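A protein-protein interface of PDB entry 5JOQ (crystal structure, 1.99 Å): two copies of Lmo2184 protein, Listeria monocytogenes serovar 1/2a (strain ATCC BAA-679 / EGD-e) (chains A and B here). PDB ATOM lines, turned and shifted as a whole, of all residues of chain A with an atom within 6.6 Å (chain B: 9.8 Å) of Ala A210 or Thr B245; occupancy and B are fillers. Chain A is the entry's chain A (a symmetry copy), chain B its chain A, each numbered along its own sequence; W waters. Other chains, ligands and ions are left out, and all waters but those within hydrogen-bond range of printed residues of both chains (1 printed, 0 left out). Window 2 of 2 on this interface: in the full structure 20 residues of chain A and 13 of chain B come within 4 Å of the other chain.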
ATOM      1  N   SER A 178       5.156  34.257 -19.204  1.00  0.00           N
ATOM      2  CA  SER A 178       4.157  33.193 -19.298  1.00  0.00           C
ATOM      3  C   SER A 178       3.214  33.365 -20.493  1.00  0.00           C
ATOM      4  O   SER A 178       2.092  32.845 -20.467  1.00  0.00           O
ATOM      5  CB  SER A 178       3.343  33.098 -18.000  1.00  0.00           C
ATOM      6  OG  SER A 178       2.864  34.378 -17.602  1.00  0.00           O
ATOM      7  N   TYR A 179       3.650  34.052 -21.555  1.00  0.00           N
ATOM      8  CA  TYR A 179       2.788  34.275 -22.718  1.00  0.00           C
ATOM      9  C   TYR A 179       2.366  32.942 -23.322  1.00  0.00           C
ATOM     10  O   TYR A 179       3.209  32.063 -23.539  1.00  0.00           O
ATOM     11  CB  TYR A 179       3.514  35.077 -23.793  1.00  0.00           C
ATOM     12  CG  TYR A 179       3.798  36.498 -23.391  1.00  0.00           C
ATOM     13  CD1 TYR A 179       2.756  37.405 -23.210  1.00  0.00           C
ATOM     14  CD2 TYR A 179       5.114  36.936 -23.213  1.00  0.00           C
ATOM     15  CE1 TYR A 179       3.019  38.735 -22.854  1.00  0.00           C
ATOM     16  CE2 TYR A 179       5.383  38.256 -22.884  1.00  0.00           C
ATOM     17  CZ  TYR A 179       4.336  39.146 -22.680  1.00  0.00           C
ATOM     18  OH  TYR A 179       4.594  40.449 -22.327  1.00  0.00           O
ATOM     19  N   LEU A 180       1.070  32.811 -23.615  1.00  0.00           N
ATOM     20  CA  LEU A 180       0.543  31.716 -24.424  1.00  0.00           C
ATOM     21  C   LEU A 180       0.463  32.133 -25.892  1.00  0.00           C
ATOM     22  O   LEU A 180       0.136  33.277 -26.203  1.00  0.00           O
ATOM     23  CB  LEU A 180      -0.867  31.334 -23.967  1.00  0.00           C
ATOM     24  CG  LEU A 180      -0.912  30.722 -22.556  1.00  0.00           C
ATOM     25  CD1 LEU A 180      -2.354  30.600 -22.097  1.00  0.00           C
ATOM     26  CD2 LEU A 180      -0.278  29.336 -22.580  1.00  0.00           C
ATOM     27  N   VAL A 181       0.692  31.170 -26.791  1.00  0.00           N
ATOM     28  CA  VAL A 181       0.434  31.383 -28.217  1.00  0.00           C
ATOM     29  C   VAL A 181      -1.038  31.109 -28.501  1.00  0.00           C
ATOM     30  O   VAL A 181      -1.572  30.077 -28.080  1.00  0.00           O
ATOM     31  CB  VAL A 181       1.332  30.473 -29.053  1.00  0.00           C
ATOM     32  CG1 VAL A 181       1.018  30.661 -30.533  1.00  0.00           C
ATOM     33  CG2 VAL A 181       2.793  30.823 -28.776  1.00  0.00           C
ATOM     34  N   TYR A 208      -4.865  27.408 -26.967  1.00  0.00           N
ATOM     35  CA  TYR A 208      -3.687  28.102 -26.421  1.00  0.00           C
ATOM     36  C   TYR A 208      -2.545  27.111 -26.277  1.00  0.00           C
ATOM     37  O   TYR A 208      -2.744  25.981 -25.805  1.00  0.00           O
ATOM     38  CB  TYR A 208      -3.974  28.757 -25.044  1.00  0.00           C
ATOM     39  CG  TYR A 208      -5.204  29.620 -25.082  1.00  0.00           C
ATOM     40  CD1 TYR A 208      -5.213  30.810 -25.810  1.00  0.00           C
ATOM     41  CD2 TYR A 208      -6.359  29.239 -24.413  1.00  0.00           C
ATOM     42  CE1 TYR A 208      -6.363  31.580 -25.892  1.00  0.00           C
ATOM     43  CE2 TYR A 208      -7.511  29.998 -24.495  1.00  0.00           C
ATOM     44  CZ  TYR A 208      -7.490  31.180 -25.232  1.00  0.00           C
ATOM     45  OH  TYR A 208      -8.643  31.916 -25.298  1.00  0.00           O
ATOM     46  N   LEU A 209      -1.362  27.514 -26.733  1.00  0.00           N
ATOM     47  CA  LEU A 209      -0.155  26.700 -26.667  1.00  0.00           C
ATOM     48  C   LEU A 209       0.880  27.372 -25.780  1.00  0.00           C
ATOM     49  O   LEU A 209       0.960  28.604 -25.706  1.00  0.00           O
ATOM     50  CB  LEU A 209       0.490  26.514 -28.066  1.00  0.00           C
ATOM     51  CG  LEU A 209      -0.304  25.770 -29.116  1.00  0.00           C
ATOM     52  CD1 LEU A 209       0.172  26.155 -30.493  1.00  0.00           C
ATOM     53  CD2 LEU A 209      -0.107  24.287 -28.884  1.00  0.00           C
ATOM     54  N   ALA A 210       1.723  26.556 -25.170  1.00  0.00           N
ATOM     55  CA  ALA A 210       2.924  27.088 -24.540  1.00  0.00           C
ATOM     56  C   ALA A 210       3.848  27.647 -25.625  1.00  0.00           C
ATOM     57  O   ALA A 210       3.905  27.129 -26.737  1.00  0.00           O
ATOM     58  CB  ALA A 210       3.636  25.990 -23.745  1.00  0.00           C
ATOM     59  N   SER A 211       4.542  28.738 -25.331  1.00  0.00           N
ATOM     60  CA  SER A 211       5.341  29.390 -26.370  1.00  0.00           C
ATOM     61  C   SER A 211       6.660  28.639 -26.553  1.00  0.00           C
ATOM     62  O   SER A 211       7.345  28.335 -25.576  1.00  0.00           O
ATOM     63  CB  SER A 211       5.587  30.852 -26.002  1.00  0.00           C
ATOM     64  OG  SER A 211       6.230  30.889 -24.722  1.00  0.00           O
ATOM     65  N   ASN A 212       6.984  28.267 -27.796  1.00  0.00           N
ATOM     66  CA  ASN A 212       8.320  27.769 -28.147  1.00  0.00           C
ATOM     67  C   ASN A 212       8.992  28.928 -28.873  1.00  0.00           C
ATOM     68  O   ASN A 212       8.811  29.120 -30.071  1.00  0.00           O
ATOM     69  CB  ASN A 212       8.264  26.517 -29.017  1.00  0.00           C
ATOM     70  CG  ASN A 212       9.669  25.951 -29.366  1.00  0.00           C
ATOM     71  OD1 ASN A 212      10.702  26.674 -29.461  1.00  0.00           O
ATOM     72  ND2 ASN A 212       9.693  24.645 -29.602  1.00  0.00           N
ATOM     73  N   THR A 213       9.736  29.741 -28.124  1.00  0.00           N
ATOM     74  CA  THR A 213      10.136  31.052 -28.674  1.00  0.00           C
ATOM     75  C   THR A 213      11.210  30.949 -29.753  1.00  0.00           C
ATOM     76  O   THR A 213      11.205  31.749 -30.703  1.00  0.00           O
ATOM     77  CB  THR A 213      10.609  31.981 -27.568  1.00  0.00           C
ATOM     78  OG1 THR A 213      11.681  31.354 -26.859  1.00  0.00           O
ATOM     79  CG2 THR A 213       9.449  32.232 -26.617  1.00  0.00           C
ATOM     80  N   LEU A 216       9.409  30.214 -32.807  1.00  0.00           N
ATOM     81  CA  LEU A 216       8.652  31.387 -33.252  1.00  0.00           C
ATOM     82  C   LEU A 216       9.580  32.432 -33.862  1.00  0.00           C
ATOM     83  O   LEU A 216       9.238  33.071 -34.867  1.00  0.00           O
ATOM     84  CB  LEU A 216       7.869  31.982 -32.085  1.00  0.00           C
ATOM     85  CG  LEU A 216       6.733  31.071 -31.526  1.00  0.00           C
ATOM     86  CD1 LEU A 216       6.178  31.652 -30.237  1.00  0.00           C
ATOM     87  CD2 LEU A 216       5.560  30.918 -32.547  1.00  0.00           C
ATOM     88  N   PRO B 176       1.738  33.551 -12.633  1.00  0.00           N
ATOM     89  CA  PRO B 176       2.544  32.540 -13.328  1.00  0.00           C
ATOM     90  C   PRO B 176       4.028  32.831 -13.204  1.00  0.00           C
ATOM     91  O   PRO B 176       4.458  33.981 -13.288  1.00  0.00           O
ATOM     92  CB  PRO B 176       2.067  32.650 -14.787  1.00  0.00           C
ATOM     93  CG  PRO B 176       0.658  33.117 -14.669  1.00  0.00           C
ATOM     94  CD  PRO B 176       0.649  34.062 -13.483  1.00  0.00           C
ATOM     95  N   ARG B 226      -5.680  28.405  -5.760  1.00  0.00           N
ATOM     96  CA  ARG B 226      -4.841  29.531  -6.172  1.00  0.00           C
ATOM     97  C   ARG B 226      -5.475  30.839  -5.727  1.00  0.00           C
ATOM     98  O   ARG B 226      -6.695  30.987  -5.763  1.00  0.00           O
ATOM     99  CB  ARG B 226      -4.644  29.568  -7.721  1.00  0.00           C
ATOM    100  CG  ARG B 226      -3.919  28.317  -8.297  1.00  0.00           C
ATOM    101  CD  ARG B 226      -3.748  28.462  -9.866  1.00  0.00           C
ATOM    102  NE  ARG B 226      -5.067  28.546 -10.527  1.00  0.00           N
ATOM    103  CZ  ARG B 226      -5.371  27.920 -11.656  1.00  0.00           C
ATOM    104  NH1 ARG B 226      -4.453  27.159 -12.247  1.00  0.00           N
ATOM    105  NH2 ARG B 226      -6.590  28.014 -12.176  1.00  0.00           N
ATOM    106  N   LYS B 237      -8.435  34.355 -15.045  1.00  0.00           N
ATOM    107  CA  LYS B 237      -8.866  33.356 -16.008  1.00  0.00           C
ATOM    108  C   LYS B 237      -7.755  33.082 -17.010  1.00  0.00           C
ATOM    109  O   LYS B 237      -7.499  31.973 -17.358  1.00  0.00           O
ATOM    110  CB  LYS B 237     -10.146  33.761 -16.722  1.00  0.00           C
ATOM    111  CG  LYS B 237     -10.677  32.689 -17.655  1.00  0.00           C
ATOM    112  CD  LYS B 237     -10.747  31.329 -16.992  1.00  0.00           C
ATOM    113  CE  LYS B 237     -11.177  30.242 -17.962  1.00  0.00           C
ATOM    114  NZ  LYS B 237     -11.222  28.876 -17.393  1.00  0.00           N
ATOM    115  N   MET B 238      -7.083  34.129 -17.440  1.00  0.00           N
ATOM    116  CA  MET B 238      -5.990  34.026 -18.371  1.00  0.00           C
ATOM    117  C   MET B 238      -4.882  33.181 -17.724  1.00  0.00           C
ATOM    118  O   MET B 238      -4.290  32.335 -18.355  1.00  0.00           O
ATOM    119  CB  MET B 238      -5.520  35.446 -18.682  1.00  0.00           C
ATOM    120  CG  MET B 238      -4.373  35.621 -19.636  1.00  0.00           C
ATOM    121  SD  MET B 238      -4.228  37.324 -20.223  1.00  0.00           S
ATOM    122  CE  MET B 238      -3.904  38.236 -18.735  1.00  0.00           C
ATOM    123  N   PHE B 239      -4.633  33.410 -16.441  1.00  0.00           N
ATOM    124  CA  PHE B 239      -3.618  32.655 -15.733  1.00  0.00           C
ATOM    125  C   PHE B 239      -4.020  31.181 -15.715  1.00  0.00           C
ATOM    126  O   PHE B 239      -3.195  30.330 -15.867  1.00  0.00           O
ATOM    127  CB  PHE B 239      -3.454  33.119 -14.289  1.00  0.00           C
ATOM    128  CG  PHE B 239      -2.848  34.491 -14.122  1.00  0.00           C
ATOM    129  CD1 PHE B 239      -2.236  35.171 -15.160  1.00  0.00           C
ATOM    130  CD2 PHE B 239      -2.872  35.082 -12.881  1.00  0.00           C
ATOM    131  CE1 PHE B 239      -1.697  36.421 -14.944  1.00  0.00           C
ATOM    132  CE2 PHE B 239      -2.333  36.319 -12.664  1.00  0.00           C
ATOM    133  CZ  PHE B 239      -1.737  36.987 -13.696  1.00  0.00           C
ATOM    134  N   ASP B 240      -5.308  30.924 -15.525  1.00  0.00           N
ATOM    135  CA  ASP B 240      -5.831  29.550 -15.490  1.00  0.00           C
ATOM    136  C   ASP B 240      -5.493  28.827 -16.781  1.00  0.00           C
ATOM    137  O   ASP B 240      -5.057  27.664 -16.766  1.00  0.00           O
ATOM    138  CB  ASP B 240      -7.350  29.558 -15.253  1.00  0.00           C
ATOM    139  CG  ASP B 240      -7.978  28.149 -15.398  1.00  0.00           C
ATOM    140  OD1 ASP B 240      -7.615  27.256 -14.612  1.00  0.00           O
ATOM    141  OD2 ASP B 240      -8.774  27.952 -16.347  1.00  0.00           O
ATOM    142  N   GLU B 241      -5.721  29.487 -17.930  1.00  0.00           N
ATOM    143  CA  GLU B 241      -5.342  28.866 -19.195  1.00  0.00           C
ATOM    144  C   GLU B 241      -3.836  28.604 -19.266  1.00  0.00           C
ATOM    145  O   GLU B 241      -3.404  27.610 -19.850  1.00  0.00           O
ATOM    146  CB  GLU B 241      -5.744  29.742 -20.395  1.00  0.00           C
ATOM    147  CG  GLU B 241      -7.204  30.042 -20.504  1.00  0.00           C
ATOM    148  CD  GLU B 241      -8.072  28.841 -20.866  1.00  0.00           C
ATOM    149  OE1 GLU B 241      -7.594  27.794 -21.366  1.00  0.00           O
ATOM    150  OE2 GLU B 241      -9.282  28.984 -20.667  1.00  0.00           O
ATOM    151  N   GLU B 242      -3.023  29.506 -18.718  1.00  0.00           N
ATOM    152  CA  GLU B 242      -1.580  29.308 -18.809  1.00  0.00           C
ATOM    153  C   GLU B 242      -1.135  28.109 -17.965  1.00  0.00           C
ATOM    154  O   GLU B 242      -0.317  27.291 -18.407  1.00  0.00           O
ATOM    155  CB  GLU B 242      -0.851  30.584 -18.364  1.00  0.00           C
ATOM    156  CG  GLU B 242       0.661  30.560 -18.755  1.00  0.00           C
ATOM    157  CD  GLU B 242       1.551  29.638 -17.865  1.00  0.00           C
ATOM    158  OE1 GLU B 242       1.283  29.484 -16.654  1.00  0.00           O
ATOM    159  OE2 GLU B 242       2.546  29.085 -18.402  1.00  0.00           O
ATOM    160  N   PHE B 243      -1.709  27.973 -16.773  1.00  0.00           N
ATOM    161  CA  PHE B 243      -1.360  26.878 -15.855  1.00  0.00           C
ATOM    162  C   PHE B 243      -1.505  25.518 -16.525  1.00  0.00           C
ATOM    163  O   PHE B 243      -0.606  24.663 -16.415  1.00  0.00           O
ATOM    164  CB  PHE B 243      -2.267  26.988 -14.620  1.00  0.00           C
ATOM    165  CG  PHE B 243      -1.750  26.319 -13.343  1.00  0.00           C
ATOM    166  CD1 PHE B 243      -0.964  27.042 -12.428  1.00  0.00           C
ATOM    167  CD2 PHE B 243      -2.159  25.040 -13.006  1.00  0.00           C
ATOM    168  CE1 PHE B 243      -0.543  26.444 -11.197  1.00  0.00           C
ATOM    169  CE2 PHE B 243      -1.762  24.438 -11.783  1.00  0.00           C
ATOM    170  CZ  PHE B 243      -0.951  25.135 -10.893  1.00  0.00           C
ATOM    171  N   LYS B 244      -2.614  25.314 -17.269  1.00  0.00           N
ATOM    172  CA  LYS B 244      -2.910  24.047 -17.936  1.00  0.00           C
ATOM    173  C   LYS B 244      -1.929  23.694 -19.050  1.00  0.00           C
ATOM    174  O   LYS B 244      -1.875  22.523 -19.454  1.00  0.00           O
ATOM    175  CB  LYS B 244      -4.330  24.078 -18.549  1.00  0.00           C
ATOM    176  CG  LYS B 244      -5.443  24.281 -17.524  1.00  0.00           C
ATOM    177  CD  LYS B 244      -6.853  24.224 -18.167  1.00  0.00           C
ATOM    178  CE  LYS B 244      -7.282  25.543 -18.786  1.00  0.00           C
ATOM    179  NZ  LYS B 244      -8.594  25.443 -19.524  1.00  0.00           N
ATOM    180  N   THR B 245      -1.229  24.671 -19.633  1.00  0.00           N
ATOM    181  CA  THR B 245      -0.271  24.393 -20.718  1.00  0.00           C
ATOM    182  C   THR B 245       1.160  24.258 -20.230  1.00  0.00           C
ATOM    183  O   THR B 245       2.049  23.941 -21.028  1.00  0.00           O
ATOM    184  CB  THR B 245      -0.272  25.517 -21.754  1.00  0.00           C
ATOM    185  OG1 THR B 245       0.403  26.660 -21.172  1.00  0.00           O
ATOM    186  CG2 THR B 245      -1.696  25.871 -22.139  1.00  0.00           C
ATOM    187  N   ASN B 246       1.403  24.528 -18.959  1.00  0.00           N
ATOM    188  CA  ASN B 246       2.744  24.683 -18.425  1.00  0.00           C
ATOM    189  C   ASN B 246       3.290  23.325 -17.998  1.00  0.00           C
ATOM    190  O   ASN B 246       2.741  22.701 -17.084  1.00  0.00           O
ATOM    191  CB  ASN B 246       2.673  25.643 -17.235  1.00  0.00           C
ATOM    192  CG  ASN B 246       4.027  26.103 -16.774  1.00  0.00           C
ATOM    193  OD1 ASN B 246       5.030  25.371 -16.888  1.00  0.00           O
ATOM    194  ND2 ASN B 246       4.071  27.325 -16.220  1.00  0.00           N
ATOM    195  N   ASP B 247       4.390  22.880 -18.616  1.00  0.00           N
ATOM    196  CA  ASP B 247       4.998  21.611 -18.193  1.00  0.00           C
ATOM    197  C   ASP B 247       5.202  21.548 -16.688  1.00  0.00           C
ATOM    198  O   ASP B 247       5.160  20.464 -16.097  1.00  0.00           O
ATOM    199  CB  ASP B 247       6.339  21.408 -18.880  1.00  0.00           C
ATOM    200  CG  ASP B 247       6.173  21.009 -20.349  1.00  0.00           C
ATOM    201  OD1 ASP B 247       5.166  20.355 -20.684  1.00  0.00           O
ATOM    202  OD2 ASP B 247       7.040  21.340 -21.132  1.00  0.00           O
ATOM    203  N   ILE B 248       5.437  22.695 -16.087  1.00  0.00           N
ATOM    204  CA  ILE B 248       5.693  22.763 -14.673  1.00  0.00           C
ATOM    205  C   ILE B 248       4.537  22.218 -13.831  1.00  0.00           C
ATOM    206  O   ILE B 248       4.789  21.632 -12.826  1.00  0.00           O
ATOM    207  CB  ILE B 248       5.971  24.222 -14.235  1.00  0.00           C
ATOM    208  CG1 ILE B 248       7.148  24.810 -15.014  1.00  0.00           C
ATOM    209  CG2 ILE B 248       6.246  24.320 -12.752  1.00  0.00           C
ATOM    210  CD1 ILE B 248       8.413  24.038 -14.798  1.00  0.00           C
ATOM    211  N   TRP B 249       3.293  22.457 -14.218  1.00  0.00           N
ATOM    212  CA  TRP B 249       2.129  22.026 -13.449  1.00  0.00           C
ATOM    213  C   TRP B 249       1.161  21.024 -14.080  1.00  0.00           C
ATOM    214  O   TRP B 249       0.419  20.345 -13.380  1.00  0.00           O
ATOM    215  CB  TRP B 249       1.289  23.270 -13.109  1.00  0.00           C
ATOM    216  CG  TRP B 249       2.004  24.368 -12.392  1.00  0.00           C
ATOM    217  CD1 TRP B 249       2.424  25.532 -12.914  1.00  0.00           C
ATOM    218  CD2 TRP B 249       2.373  24.388 -11.018  1.00  0.00           C
ATOM    219  NE1 TRP B 249       3.034  26.288 -11.967  1.00  0.00           N
ATOM    220  CE2 TRP B 249       3.025  25.604 -10.786  1.00  0.00           C
ATOM    221  CE3 TRP B 249       2.235  23.488  -9.967  1.00  0.00           C
ATOM    222  CZ2 TRP B 249       3.527  25.946  -9.551  1.00  0.00           C
ATOM    223  CZ3 TRP B 249       2.731  23.825  -8.749  1.00  0.00           C
ATOM    224  CH2 TRP B 249       3.365  25.051  -8.540  1.00  0.00           C
ATOM    225  N   LYS B 250       1.174  20.955 -15.401  1.00  0.00           N
ATOM    226  CA  LYS B 250       0.220  20.156 -16.145  1.00  0.00           C
ATOM    227  C   LYS B 250       0.218  18.666 -15.919  1.00  0.00           C
ATOM    228  O   LYS B 250      -0.734  18.016 -16.218  1.00  0.00           O
ATOM    229  CB  LYS B 250       0.176  20.504 -17.623  1.00  0.00           C
ATOM    230  CG  LYS B 250       1.258  19.910 -18.477  1.00  0.00           C
ATOM    231  CD  LYS B 250       0.924  20.207 -19.922  1.00  0.00           C
ATOM    232  CE  LYS B 250       1.928  19.638 -20.879  1.00  0.00           C
ATOM    233  NZ  LYS B 250       1.355  19.653 -22.247  1.00  0.00           N
ATOM    234  N   HIS B 251       1.300  18.125 -15.423  1.00  0.00           N
ATOM    235  CA  HIS B 251       1.287  16.689 -15.140  1.00  0.00           C
ATOM    236  C   HIS B 251       0.875  16.371 -13.697  1.00  0.00           C
ATOM    237  O   HIS B 251       0.818  15.190 -13.332  1.00  0.00           O
ATOM    238  CB  HIS B 251       2.638  16.081 -15.488  1.00  0.00           C
ATOM    239  CG  HIS B 251       3.081  16.421 -16.890  1.00  0.00           C
ATOM    240  ND1 HIS B 251       2.634  15.727 -17.995  1.00  0.00           N
ATOM    241  CD2 HIS B 251       3.877  17.408 -17.362  1.00  0.00           C
ATOM    242  CE1 HIS B 251       3.145  16.263 -19.087  1.00  0.00           C
ATOM    243  NE2 HIS B 251       3.906  17.286 -18.729  1.00  0.00           N
ATOM    244  N   VAL B 255      -4.464  18.783 -11.806  1.00  0.00           N
ATOM    245  CA  VAL B 255      -4.770  19.414 -13.092  1.00  0.00           C
ATOM    246  C   VAL B 255      -5.502  18.431 -14.005  1.00  0.00           C
ATOM    247  O   VAL B 255      -6.556  18.746 -14.574  1.00  0.00           O
ATOM    248  CB  VAL B 255      -3.493  19.949 -13.746  1.00  0.00           C
ATOM    249  CG1 VAL B 255      -3.824  20.523 -15.138  1.00  0.00           C
ATOM    250  CG2 VAL B 255      -2.867  21.025 -12.818  1.00  0.00           C
HETATM  251  O   HOH W   1       5.623  34.877 -15.879  1.00  0.00           O
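NZ of Lys B237 is in salt-bridge range of OE2 of Glu B241 (3.8 Å).
The side-chain carboxylate (OE1) of Glu B241 is in salt-bridge range of the side-chain amino group (NZ) of Lys B244, at 3.1 Å.
O of Glu B242 is in hydrogen-bond range of OG1 of Thr B245 (2.9 Å).
The side-chain carboxylate of Glu B242 lies within hydrogen-bond range of the side-chain amide nitrogen of Asn B246, 3.2 Å away.
Among the printed residues, pairs that only touch across the chains: Leu A180 with Thr B245 (3.1 Å), Ser A178 with Glu B242 (3.2 Å), Ser A178 with Pro B176 (3.4 Å), Tyr A208 with Glu B241 (3.6 Å), Leu A180 with Glu B242 (3.6 Å), Ala A210 with Thr B245 (3.8 Å), Leu A180 with Glu B241 (3.8 Å) and Tyr A208 with Thr B245 (3.8 Å).
Of chain B, only Thr B245 (3.8 Å) comes within 4 Å of Ala A210.
Thr B245 touches three residues of chain A.
Of the printed residues of chain A, Glu B242 touches Ser A178 and Leu A180.
Of the printed residues of chain B, Leu A180 touches Glu B241, Glu B242 and Thr B245.
Printed residues of chain B within 4 Å of Tyr A208: Glu B241 and Thr B245.
Of the printed residues of chain B, Ser A178 touches Pro B176 (3.4 Å) and Glu B242 (3.2 Å).
The nearest printed residue of chain A that does not touch Thr B245 is Leu A209 (4.6 Å).
The nearest printed residue of chain B that does not touch Leu A180 is Met B238 (4.6 Å).
Of the 18 printed residues of chain B, 4 touch a printed residue of chain A.
Of the 11 printed residues of chain A, 4 touch a printed residue of chain B.
Hydrophobic or aromatic side chains of chain A that line the printed part of chain B: Leu A180, Tyr A208 and Ala A210.
Among the printed residues, no Asp or Glu carboxylate lies within 4 Å of a Lys or Arg side-chain nitrogen of the other chain.
No position is printed for both chains.
Of the 8 pairs that touch across the chains among the printed residues, none has its exchanged pair printed and touching as well.
Water W1 bridges the backbone carbonyl oxygen (O) of Pro B176 (3.0 Å) and the side-chain hydroxyl (OG) of Ser A178 (3.3 Å).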
